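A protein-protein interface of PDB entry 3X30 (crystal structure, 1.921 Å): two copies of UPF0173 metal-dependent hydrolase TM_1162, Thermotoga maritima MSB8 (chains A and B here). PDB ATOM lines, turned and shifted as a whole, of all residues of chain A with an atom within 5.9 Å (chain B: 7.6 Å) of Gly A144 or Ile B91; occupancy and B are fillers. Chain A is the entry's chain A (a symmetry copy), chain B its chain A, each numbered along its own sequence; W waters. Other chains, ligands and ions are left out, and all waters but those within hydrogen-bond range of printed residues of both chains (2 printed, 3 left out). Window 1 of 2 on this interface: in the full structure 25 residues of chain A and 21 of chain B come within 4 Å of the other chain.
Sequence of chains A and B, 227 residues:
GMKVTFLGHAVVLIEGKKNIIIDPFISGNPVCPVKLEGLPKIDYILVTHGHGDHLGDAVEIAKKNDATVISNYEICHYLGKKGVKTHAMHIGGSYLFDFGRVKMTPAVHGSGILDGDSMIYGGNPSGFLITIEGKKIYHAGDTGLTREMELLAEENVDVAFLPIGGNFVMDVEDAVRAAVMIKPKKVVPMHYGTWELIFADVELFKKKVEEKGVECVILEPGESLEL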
ATOM      1  N   ALA A 107     -25.542   2.119  12.485  1.00  0.00           N
ATOM      2  CA  ALA A 107     -25.204   0.706  12.349  1.00  0.00           C
ATOM      3  C   ALA A 107     -26.207   0.095  11.381  1.00  0.00           C
ATOM      4  O   ALA A 107     -27.297   0.656  11.168  1.00  0.00           O
ATOM      5  CB  ALA A 107     -25.244  -0.010  13.715  1.00  0.00           C
ATOM      6  N   VAL A 108     -25.869  -1.039  10.783  1.00  0.00           N
ATOM      7  CA  VAL A 108     -26.873  -1.751   9.994  1.00  0.00           C
ATOM      8  C   VAL A 108     -27.135  -3.091  10.701  1.00  0.00           C
ATOM      9  O   VAL A 108     -26.268  -3.943  10.805  1.00  0.00           O
ATOM     10  CB  VAL A 108     -26.451  -1.890   8.494  1.00  0.00           C
ATOM     11  CG1 VAL A 108     -26.396  -0.504   7.854  1.00  0.00           C
ATOM     12  CG2 VAL A 108     -25.103  -2.617   8.300  1.00  0.00           C
ATOM     13  N   HIS A 109     -28.337  -3.229  11.250  1.00  0.00           N
ATOM     14  CA  HIS A 109     -28.626  -4.328  12.176  1.00  0.00           C
ATOM     15  C   HIS A 109     -30.119  -4.242  12.508  1.00  0.00           C
ATOM     16  O   HIS A 109     -30.898  -3.688  11.722  1.00  0.00           O
ATOM     17  CB  HIS A 109     -27.724  -4.208  13.440  1.00  0.00           C
ATOM     18  CG  HIS A 109     -27.681  -5.437  14.299  1.00  0.00           C
ATOM     19  ND1 HIS A 109     -27.146  -6.632  13.871  1.00  0.00           N
ATOM     20  CD2 HIS A 109     -28.094  -5.644  15.576  1.00  0.00           C
ATOM     21  CE1 HIS A 109     -27.246  -7.528  14.840  1.00  0.00           C
ATOM     22  NE2 HIS A 109     -27.812  -6.952  15.887  1.00  0.00           N
ATOM     23  N   GLY A 110     -30.517  -4.779  13.659  1.00  0.00           N
ATOM     24  CA  GLY A 110     -31.879  -4.624  14.144  1.00  0.00           C
ATOM     25  C   GLY A 110     -31.862  -4.202  15.599  1.00  0.00           C
ATOM     26  O   GLY A 110     -30.796  -4.160  16.213  1.00  0.00           O
ATOM     27  N   ASP A 142     -23.552  -4.012  17.360  1.00  0.00           N
ATOM     28  CA  ASP A 142     -23.742  -5.024  16.330  1.00  0.00           C
ATOM     29  C   ASP A 142     -23.996  -4.320  15.009  1.00  0.00           C
ATOM     30  O   ASP A 142     -24.860  -3.448  14.916  1.00  0.00           O
ATOM     31  CB  ASP A 142     -24.926  -5.936  16.619  1.00  0.00           C
ATOM     32  CG  ASP A 142     -24.616  -7.055  17.592  1.00  0.00           C
ATOM     33  OD1 ASP A 142     -23.457  -7.213  18.024  1.00  0.00           O
ATOM     34  OD2 ASP A 142     -25.577  -7.777  17.928  1.00  0.00           O
ATOM     35  N   THR A 143     -23.278  -4.717  13.972  1.00  0.00           N
ATOM     36  CA  THR A 143     -23.470  -4.085  12.688  1.00  0.00           C
ATOM     37  C   THR A 143     -22.812  -4.917  11.599  1.00  0.00           C
ATOM     38  O   THR A 143     -21.897  -5.708  11.866  1.00  0.00           O
ATOM     39  CB  THR A 143     -22.896  -2.639  12.668  1.00  0.00           C
ATOM     40  OG1 THR A 143     -23.205  -2.017  11.414  1.00  0.00           O
ATOM     41  CG2 THR A 143     -21.385  -2.652  12.869  1.00  0.00           C
ATOM     42  N   GLY A 144     -23.326  -4.759  10.385  1.00  0.00           N
ATOM     43  CA  GLY A 144     -22.648  -5.229   9.202  1.00  0.00           C
ATOM     44  C   GLY A 144     -21.816  -4.083   8.666  1.00  0.00           C
ATOM     45  O   GLY A 144     -21.813  -2.969   9.207  1.00  0.00           O
ATOM     46  N   LEU A 145     -21.106  -4.362   7.588  1.00  0.00           N
ATOM     47  CA  LEU A 145     -20.305  -3.357   6.917  1.00  0.00           C
ATOM     48  C   LEU A 145     -21.224  -2.271   6.346  1.00  0.00           C
ATOM     49  O   LEU A 145     -22.217  -2.580   5.701  1.00  0.00           O
ATOM     50  CB  LEU A 145     -19.483  -4.013   5.810  1.00  0.00           C
ATOM     51  CG  LEU A 145     -18.509  -3.093   5.072  1.00  0.00           C
ATOM     52  CD1 LEU A 145     -17.468  -2.575   6.051  1.00  0.00           C
ATOM     53  CD2 LEU A 145     -17.862  -3.877   3.933  1.00  0.00           C
ATOM     54  N   THR A 146     -20.898  -1.008   6.597  1.00  0.00           N
ATOM     55  CA  THR A 146     -21.689   0.092   6.060  1.00  0.00           C
ATOM     56  C   THR A 146     -20.784   1.267   5.687  1.00  0.00           C
ATOM     57  O   THR A 146     -19.797   1.557   6.374  1.00  0.00           O
ATOM     58  CB  THR A 146     -22.769   0.563   7.065  1.00  0.00           C
ATOM     59  OG1 THR A 146     -23.276   1.833   6.651  1.00  0.00           O
ATOM     60  CG2 THR A 146     -22.187   0.701   8.466  1.00  0.00           C
ATOM     61  N   MET A 149     -19.471   4.108   8.094  1.00  0.00           N
ATOM     62  CA  MET A 149     -18.220   4.027   8.845  1.00  0.00           C
ATOM     63  C   MET A 149     -17.138   4.954   8.285  1.00  0.00           C
ATOM     64  O   MET A 149     -16.254   5.394   9.011  1.00  0.00           O
ATOM     65  CB  MET A 149     -17.712   2.587   8.866  1.00  0.00           C
ATOM     66  CG  MET A 149     -18.574   1.693   9.725  1.00  0.00           C
ATOM     67  SD  MET A 149     -18.272  -0.178   9.270  1.00  0.00           S
ATOM     68  CE  MET A 149     -19.301  -0.960  10.750  1.00  0.00           C
ATOM     69  N   ASN A 167     -22.354 -14.009  10.869  1.00  0.00           N
ATOM     70  CA  ASN A 167     -23.772 -14.405  10.965  1.00  0.00           C
ATOM     71  C   ASN A 167     -24.752 -13.289  11.364  1.00  0.00           C
ATOM     72  O   ASN A 167     -25.610 -12.912  10.562  1.00  0.00           O
ATOM     73  CB  ASN A 167     -23.978 -15.589  11.924  1.00  0.00           C
ATOM     74  CG  ASN A 167     -25.364 -16.204  11.764  1.00  0.00           C
ATOM     75  OD1 ASN A 167     -25.614 -16.921  10.795  1.00  0.00           O
ATOM     76  ND2 ASN A 167     -26.287 -15.877  12.675  1.00  0.00           N
ATOM     77  N   PHE A 168     -24.649 -12.804  12.601  1.00  0.00           N
ATOM     78  CA  PHE A 168     -25.435 -11.652  13.052  1.00  0.00           C
ATOM     79  C   PHE A 168     -24.719 -10.342  12.791  1.00  0.00           C
ATOM     80  O   PHE A 168     -25.344  -9.280  12.791  1.00  0.00           O
ATOM     81  CB  PHE A 168     -25.743 -11.732  14.543  1.00  0.00           C
ATOM     82  CG  PHE A 168     -26.609 -12.900  14.921  1.00  0.00           C
ATOM     83  CD1 PHE A 168     -27.937 -12.956  14.527  1.00  0.00           C
ATOM     84  CD2 PHE A 168     -26.084 -13.949  15.660  1.00  0.00           C
ATOM     85  CE1 PHE A 168     -28.738 -14.041  14.878  1.00  0.00           C
ATOM     86  CE2 PHE A 168     -26.879 -15.029  16.014  1.00  0.00           C
ATOM     87  CZ  PHE A 168     -28.200 -15.074  15.624  1.00  0.00           C
ATOM     88  N   VAL A 169     -23.404 -10.420  12.603  1.00  0.00           N
ATOM     89  CA  VAL A 169     -22.561  -9.234  12.468  1.00  0.00           C
ATOM     90  C   VAL A 169     -21.490  -9.505  11.432  1.00  0.00           C
ATOM     91  O   VAL A 169     -21.415 -10.615  10.902  1.00  0.00           O
ATOM     92  CB  VAL A 169     -21.892  -8.853  13.798  1.00  0.00           C
ATOM     93  CG1 VAL A 169     -22.953  -8.536  14.876  1.00  0.00           C
ATOM     94  CG2 VAL A 169     -20.971  -9.975  14.258  1.00  0.00           C
ATOM     95  N   MET A 170     -20.655  -8.505  11.159  1.00  0.00           N
ATOM     96  CA  MET A 170     -19.541  -8.672  10.229  1.00  0.00           C
ATOM     97  C   MET A 170     -18.713  -9.905  10.553  1.00  0.00           C
ATOM     98  O   MET A 170     -18.497 -10.211  11.725  1.00  0.00           O
ATOM     99  CB  MET A 170     -18.620  -7.449  10.266  1.00  0.00           C
ATOM    100  CG  MET A 170     -19.285  -6.152   9.877  1.00  0.00           C
ATOM    101  SD  MET A 170     -17.935  -4.757   9.664  1.00  0.00           S
ATOM    102  CE  MET A 170     -17.490  -4.507  11.547  1.00  0.00           C
ATOM    103  N   THR B  48     -36.708 -11.376   2.885  1.00  0.00           N
ATOM    104  CA  THR B  48     -35.967 -10.108   2.936  1.00  0.00           C
ATOM    105  C   THR B  48     -36.515  -9.140   3.984  1.00  0.00           C
ATOM    106  O   THR B  48     -35.753  -8.402   4.610  1.00  0.00           O
ATOM    107  CB  THR B  48     -35.984  -9.386   1.584  1.00  0.00           C
ATOM    108  OG1 THR B  48     -37.338  -9.173   1.174  1.00  0.00           O
ATOM    109  CG2 THR B  48     -35.243 -10.207   0.515  1.00  0.00           C
ATOM    110  N   SER B  71     -33.681 -15.546   7.808  1.00  0.00           N
ATOM    111  CA  SER B  71     -34.113 -14.145   7.848  1.00  0.00           C
ATOM    112  C   SER B  71     -33.452 -13.441   9.040  1.00  0.00           C
ATOM    113  O   SER B  71     -32.582 -14.022   9.684  1.00  0.00           O
ATOM    114  CB  SER B  71     -35.644 -14.050   7.931  1.00  0.00           C
ATOM    115  OG  SER B  71     -36.101 -12.751   7.551  1.00  0.00           O
ATOM    116  N   ASN B  72     -33.845 -12.201   9.340  1.00  0.00           N
ATOM    117  CA  ASN B  72     -33.233 -11.518  10.479  1.00  0.00           C
ATOM    118  C   ASN B  72     -33.790 -12.049  11.779  1.00  0.00           C
ATOM    119  O   ASN B  72     -34.776 -12.799  11.795  1.00  0.00           O
ATOM    120  CB  ASN B  72     -33.388  -9.972  10.391  1.00  0.00           C
ATOM    121  CG  ASN B  72     -34.826  -9.483  10.523  1.00  0.00           C
ATOM    122  OD1 ASN B  72     -35.595  -9.950  11.365  1.00  0.00           O
ATOM    123  ND2 ASN B  72     -35.181  -8.489   9.708  1.00  0.00           N
ATOM    124  N   TYR B  73     -33.143 -11.659  12.870  1.00  0.00           N
ATOM    125  CA  TYR B  73     -33.458 -12.190  14.179  1.00  0.00           C
ATOM    126  C   TYR B  73     -34.926 -11.996  14.532  1.00  0.00           C
ATOM    127  O   TYR B  73     -35.584 -12.915  15.000  1.00  0.00           O
ATOM    128  CB  TYR B  73     -32.541 -11.530  15.215  1.00  0.00           C
ATOM    129  CG  TYR B  73     -32.905 -11.750  16.665  1.00  0.00           C
ATOM    130  CD1 TYR B  73     -32.705 -12.978  17.284  1.00  0.00           C
ATOM    131  CD2 TYR B  73     -33.379 -10.694  17.435  1.00  0.00           C
ATOM    132  CE1 TYR B  73     -33.010 -13.155  18.639  1.00  0.00           C
ATOM    133  CE2 TYR B  73     -33.678 -10.855  18.766  1.00  0.00           C
ATOM    134  CZ  TYR B  73     -33.500 -12.080  19.366  1.00  0.00           C
ATOM    135  OH  TYR B  73     -33.823 -12.194  20.699  1.00  0.00           O
ATOM    136  N   MET B  89     -30.132 -14.524  11.182  1.00  0.00           N
ATOM    137  CA  MET B  89     -28.934 -13.766  10.868  1.00  0.00           C
ATOM    138  C   MET B  89     -29.257 -12.305  11.136  1.00  0.00           C
ATOM    139  O   MET B  89     -30.300 -12.012  11.713  1.00  0.00           O
ATOM    140  CB  MET B  89     -28.520 -13.973   9.404  1.00  0.00           C
ATOM    141  CG  MET B  89     -28.647 -15.403   8.927  1.00  0.00           C
ATOM    142  SD  MET B  89     -27.848 -15.648   7.136  1.00  0.00           S
ATOM    143  CE  MET B  89     -26.080 -15.268   7.683  1.00  0.00           C
ATOM    144  N   HIS B  90     -28.382 -11.387  10.728  1.00  0.00           N
ATOM    145  CA  HIS B  90     -28.811  -9.991  10.633  1.00  0.00           C
ATOM    146  C   HIS B  90     -27.971  -9.240   9.601  1.00  0.00           C
ATOM    147  O   HIS B  90     -27.119  -9.832   8.926  1.00  0.00           O
ATOM    148  CB  HIS B  90     -28.791  -9.263  11.997  1.00  0.00           C
ATOM    149  CG  HIS B  90     -30.027  -8.437  12.206  1.00  0.00           C
ATOM    150  ND1 HIS B  90     -30.920  -8.680  13.236  1.00  0.00           N
ATOM    151  CD2 HIS B  90     -30.590  -7.476  11.440  1.00  0.00           C
ATOM    152  CE1 HIS B  90     -31.946  -7.855  13.125  1.00  0.00           C
ATOM    153  NE2 HIS B  90     -31.776  -7.120  12.039  1.00  0.00           N
ATOM    154  N   ILE B  91     -28.258  -7.947   9.447  1.00  0.00           N
ATOM    155  CA  ILE B  91     -27.783  -7.211   8.280  1.00  0.00           C
ATOM    156  C   ILE B  91     -26.257  -7.193   8.168  1.00  0.00           C
ATOM    157  O   ILE B  91     -25.552  -6.770   9.088  1.00  0.00           O
ATOM    158  CB  ILE B  91     -28.280  -5.743   8.274  1.00  0.00           C
ATOM    159  CG1 ILE B  91     -29.782  -5.647   8.563  1.00  0.00           C
ATOM    160  CG2 ILE B  91     -27.909  -5.091   6.944  1.00  0.00           C
ATOM    161  CD1 ILE B  91     -30.643  -6.455   7.596  1.00  0.00           C
ATOM    162  N   GLY B  92     -25.746  -7.663   7.039  1.00  0.00           N
ATOM    163  CA  GLY B  92     -24.309  -7.658   6.812  1.00  0.00           C
ATOM    164  C   GLY B  92     -23.667  -8.939   7.306  1.00  0.00           C
ATOM    165  O   GLY B  92     -22.473  -9.148   7.136  1.00  0.00           O
ATOM    166  N   GLY B  93     -24.462  -9.812   7.913  1.00  0.00           N
ATOM    167  CA  GLY B  93     -23.921 -11.057   8.427  1.00  0.00           C
ATOM    168  C   GLY B  93     -24.005 -12.129   7.361  1.00  0.00           C
ATOM    169  O   GLY B  93     -24.862 -12.060   6.474  1.00  0.00           O
ATOM    170  N   SER B  94     -23.116 -13.114   7.438  1.00  0.00           N
ATOM    171  CA  SER B  94     -23.136 -14.215   6.480  1.00  0.00           C
ATOM    172  C   SER B  94     -22.875 -15.550   7.168  1.00  0.00           C
ATOM    173  O   SER B  94     -22.334 -15.606   8.279  1.00  0.00           O
ATOM    174  CB  SER B  94     -22.120 -13.995   5.358  1.00  0.00           C
ATOM    175  OG  SER B  94     -20.804 -14.088   5.850  1.00  0.00           O
ATOM    176  N   LYS B 103     -25.436 -14.106   2.506  1.00  0.00           N
ATOM    177  CA  LYS B 103     -25.139 -12.876   3.232  1.00  0.00           C
ATOM    178  C   LYS B 103     -26.344 -11.960   3.148  1.00  0.00           C
ATOM    179  O   LYS B 103     -26.916 -11.793   2.063  1.00  0.00           O
ATOM    180  CB  LYS B 103     -23.909 -12.186   2.643  1.00  0.00           C
ATOM    181  CG  LYS B 103     -23.542 -10.864   3.309  1.00  0.00           C
ATOM    182  CD  LYS B 103     -22.320 -10.275   2.616  1.00  0.00           C
ATOM    183  CE  LYS B 103     -21.683  -9.173   3.428  1.00  0.00           C
ATOM    184  NZ  LYS B 103     -20.364  -8.778   2.816  1.00  0.00           N
ATOM    185  N   MET B 104     -26.765 -11.394   4.280  1.00  0.00           N
ATOM    186  CA  MET B 104     -27.858 -10.417   4.270  1.00  0.00           C
ATOM    187  C   MET B 104     -27.242  -9.076   3.965  1.00  0.00           C
ATOM    188  O   MET B 104     -26.232  -8.717   4.556  1.00  0.00           O
ATOM    189  CB  MET B 104     -28.613 -10.344   5.617  1.00  0.00           C
ATOM    190  CG  MET B 104     -29.376 -11.577   6.005  1.00  0.00           C
ATOM    191  SD  MET B 104     -30.625 -11.096   7.462  1.00  0.00           S
ATOM    192  CE  MET B 104     -32.252 -11.029   6.378  1.00  0.00           C
ATOM    193  N   THR B 105     -27.834  -8.338   3.039  1.00  0.00           N
ATOM    194  CA  THR B 105     -27.287  -7.044   2.637  1.00  0.00           C
ATOM    195  C   THR B 105     -28.190  -5.921   3.118  1.00  0.00           C
ATOM    196  O   THR B 105     -29.381  -6.138   3.314  1.00  0.00           O
ATOM    197  CB  THR B 105     -27.159  -6.952   1.118  1.00  0.00           C
ATOM    198  OG1 THR B 105     -28.475  -7.007   0.549  1.00  0.00           O
ATOM    199  CG2 THR B 105     -26.323  -8.121   0.575  1.00  0.00           C
ATOM    200  N   PRO B 106     -27.624  -4.717   3.317  1.00  0.00           N
ATOM    201  CA  PRO B 106     -28.433  -3.559   3.715  1.00  0.00           C
ATOM    202  C   PRO B 106     -29.490  -3.210   2.673  1.00  0.00           C
ATOM    203  O   PRO B 106     -29.279  -3.403   1.467  1.00  0.00           O
ATOM    204  CB  PRO B 106     -27.391  -2.427   3.834  1.00  0.00           C
ATOM    205  CG  PRO B 106     -26.100  -3.138   4.126  1.00  0.00           C
ATOM    206  CD  PRO B 106     -26.180  -4.414   3.325  1.00  0.00           C
ATOM    207  N   ALA B 107     -30.637  -2.747   3.150  1.00  0.00           N
ATOM    208  CA  ALA B 107     -31.672  -2.172   2.296  1.00  0.00           C
ATOM    209  C   ALA B 107     -32.181  -0.918   2.992  1.00  0.00           C
ATOM    210  O   ALA B 107     -32.009  -0.763   4.213  1.00  0.00           O
ATOM    211  CB  ALA B 107     -32.816  -3.178   2.055  1.00  0.00           C
ATOM    212  N   GLY B 123     -37.694  -6.293  12.576  1.00  0.00           N
ATOM    213  CA  GLY B 123     -36.285  -5.964  12.422  1.00  0.00           C
ATOM    214  C   GLY B 123     -36.070  -4.890  11.374  1.00  0.00           C
ATOM    215  O   GLY B 123     -36.905  -4.003  11.221  1.00  0.00           O
ATOM    216  N   ASN B 124     -34.944  -4.958  10.668  1.00  0.00           N
ATOM    217  CA  ASN B 124     -34.693  -4.074   9.532  1.00  0.00           C
ATOM    218  C   ASN B 124     -34.682  -4.883   8.234  1.00  0.00           C
ATOM    219  O   ASN B 124     -34.343  -6.064   8.239  1.00  0.00           O
ATOM    220  CB  ASN B 124     -33.374  -3.310   9.707  1.00  0.00           C
ATOM    221  CG  ASN B 124     -33.579  -1.931  10.349  1.00  0.00           C
ATOM    222  OD1 ASN B 124     -34.602  -1.284  10.137  1.00  0.00           O
ATOM    223  ND2 ASN B 124     -32.612  -1.493  11.134  1.00  0.00           N
ATOM    224  N   PRO B 125     -35.074  -4.249   7.118  1.00  0.00           N
ATOM    225  CA  PRO B 125     -35.177  -4.966   5.847  1.00  0.00           C
ATOM    226  C   PRO B 125     -33.799  -5.251   5.251  1.00  0.00           C
ATOM    227  O   PRO B 125     -32.840  -4.561   5.566  1.00  0.00           O
ATOM    228  CB  PRO B 125     -35.965  -4.001   4.962  1.00  0.00           C
ATOM    229  CG  PRO B 125     -35.526  -2.619   5.476  1.00  0.00           C
ATOM    230  CD  PRO B 125     -35.374  -2.805   6.974  1.00  0.00           C
ATOM    231  N   SER B 126     -33.717  -6.260   4.389  1.00  0.00           N
ATOM    232  CA  SER B 126     -32.452  -6.634   3.791  1.00  0.00           C
ATOM    233  C   SER B 126     -32.605  -7.045   2.337  1.00  0.00           C
ATOM    234  O   SER B 126     -33.716  -7.111   1.805  1.00  0.00           O
ATOM    235  CB  SER B 126     -31.825  -7.800   4.563  1.00  0.00           C
ATOM    236  OG  SER B 126     -32.397  -9.017   4.110  1.00  0.00           O
ATOM    237  N   GLY B 127     -31.469  -7.312   1.702  1.00  0.00           N
ATOM    238  CA  GLY B 127     -31.451  -8.124   0.505  1.00  0.00           C
ATOM    239  C   GLY B 127     -30.602  -9.333   0.842  1.00  0.00           C
ATOM    240  O   GLY B 127     -30.184  -9.512   1.994  1.00  0.00           O
ATOM    241  N   GLU B 148     -24.962   1.783   0.049  1.00  0.00           N
ATOM    242  CA  GLU B 148     -24.481   0.485   0.546  1.00  0.00           C
ATOM    243  C   GLU B 148     -24.354  -0.499  -0.615  1.00  0.00           C
ATOM    244  O   GLU B 148     -23.563  -1.444  -0.567  1.00  0.00           O
ATOM    245  CB  GLU B 148     -25.413  -0.090   1.633  1.00  0.00           C
ATOM    246  CG  GLU B 148     -25.736   0.876   2.791  1.00  0.00           C
ATOM    247  CD  GLU B 148     -24.538   1.187   3.696  1.00  0.00           C
ATOM    248  OE1 GLU B 148     -23.378   0.885   3.330  1.00  0.00           O
ATOM    249  OE2 GLU B 148     -24.760   1.747   4.792  1.00  0.00           O
ATOM    250  N   LEU B 151     -20.957  -1.407  -2.087  1.00  0.00           N
ATOM    251  CA  LEU B 151     -20.136  -2.439  -1.434  1.00  0.00           C
ATOM    252  C   LEU B 151     -20.145  -3.741  -2.229  1.00  0.00           C
ATOM    253  O   LEU B 151     -19.299  -4.611  -2.012  1.00  0.00           O
ATOM    254  CB  LEU B 151     -20.626  -2.717  -0.001  1.00  0.00           C
ATOM    255  CG  LEU B 151     -20.571  -1.541   0.979  1.00  0.00           C
ATOM    256  CD1 LEU B 151     -21.175  -1.932   2.323  1.00  0.00           C
ATOM    257  CD2 LEU B 151     -19.145  -1.066   1.148  1.00  0.00           C
HETATM  258  O   HOH W   1     -20.811 -13.021   8.491  1.00  0.00           O
HETATM  259  O   HOH W   2     -21.125  -6.918   6.226  1.00  0.00           O
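A ring nitrogen (NE2) of His B90 sits at hydrogen-bond distance from the backbone NH (N) of Gly A110, at 3.1 Å.
O of Asn A167 lies within hydrogen-bond range of N of His B90 (3.2 Å).
O of Ile B91 lies within hydrogen-bond range of N of Gly A144 (3.3 Å).
The backbone carbonyl oxygen (O) of Ser B94 sits at hydrogen-bond distance from the backbone NH (N) of Asn A167 (3.0 Å).
The backbone carbonyl oxygen of His A109 sits at hydrogen-bond distance from the side-chain amide nitrogen of Asn B124, 2.8 Å away.
OE1 of Glu B148 lies close to OG1 of Thr A146 (3.5 Å).
The backbone carbonyl oxygen (O) of Val A108 sits close to the backbone carbonyl oxygen (O) of Ile B91.
The backbone carbonyl oxygen (O) of Ser B71 is in hydrogen-bond range of the backbone NH (N) of Met B89, 2.9 Å away.
The backbone carbonyl oxygen of Met B89 sits at hydrogen-bond distance from the backbone NH of Tyr B73 (3.1 Å).
The backbone carbonyl oxygen (O) of Gly B93 lies within hydrogen-bond range of the backbone NH (N) of Met B104 (3.0 Å).
The backbone NH of Val A108 sits at hydrogen-bond distance from the side-chain hydroxyl of Thr A143, at 2.9 Å.
The backbone carbonyl oxygen of Val A108 is in hydrogen-bond range of the backbone NH of Gly A144, 3.1 Å away.
The backbone carbonyl oxygen (O) of Phe A168 sits close to a ring nitrogen (ND1) of His A109 (3.4 Å).
His A109 touches His B90 (C to NE2, 3.4 Å).
O of His A109 touches CG1 of Ile B91, at 3.9 Å.
Gly A144 touches Gly B92 (CA to CA, 3.8 Å).
Leu A145 touches Leu B151.
Asn A167 touches Met B89.
Asn A167 touches Gly B93.
CD1 of Phe A168 touches C of Met B89 (3.7 Å).
O of Phe A168 touches CB of His B90, at 3.5 Å.
CA of Gly B93 touches O of Val A169, 3.5 Å away.
Of chain B, only Ile B91 and Gly B92 come within 4 Å of Gly A144.
Of chain A, only Val A108 (3.4 Å), His A109 (3.9 Å) and Gly A144 (3.3 Å) come within 4 Å of Ile B91.
Printed residues of chain A within 4 Å of Ser B94: Asn A167 (3.0 Å).
Of the printed residues of chain A, Leu B151 touches Leu A145 (3.6 Å).
Printed residues of chain A within 4 Å of Glu B148: Thr A146 (2.4 Å).
Asn B72 touches none of the printed residues of chain A.
Pro B106 touches none of the printed residues of chain A.
The nearest printed residue of chain B that does not touch Val A169 is Gly B92 (4.2 Å).
Of the 22 printed residues of chain B, 9 touch a printed residue of chain A.
Hydrophobic or aromatic side chains of chain B that line the printed part of chain A: Met B89, His B90, Ile B91 and Leu B151.
Among the printed residues, no Asp or Glu carboxylate lies within 4 Å of a Lys or Arg side-chain nitrogen of the other chain.
1 position is printed for both chains.
Of the 16 pairs that touch across the chains among the printed residues, none has its exchanged pair printed and touching as well.
Water W1 lies within hydrogen-bond range of N of Ser B94, N of Asn A167 and O of Val A169.
Water W2 lies within hydrogen-bond range of the backbone carbonyl oxygen (O) of Gly B92 (2.8 Å) and the backbone NH (N) of Leu A145 (2.9 Å).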
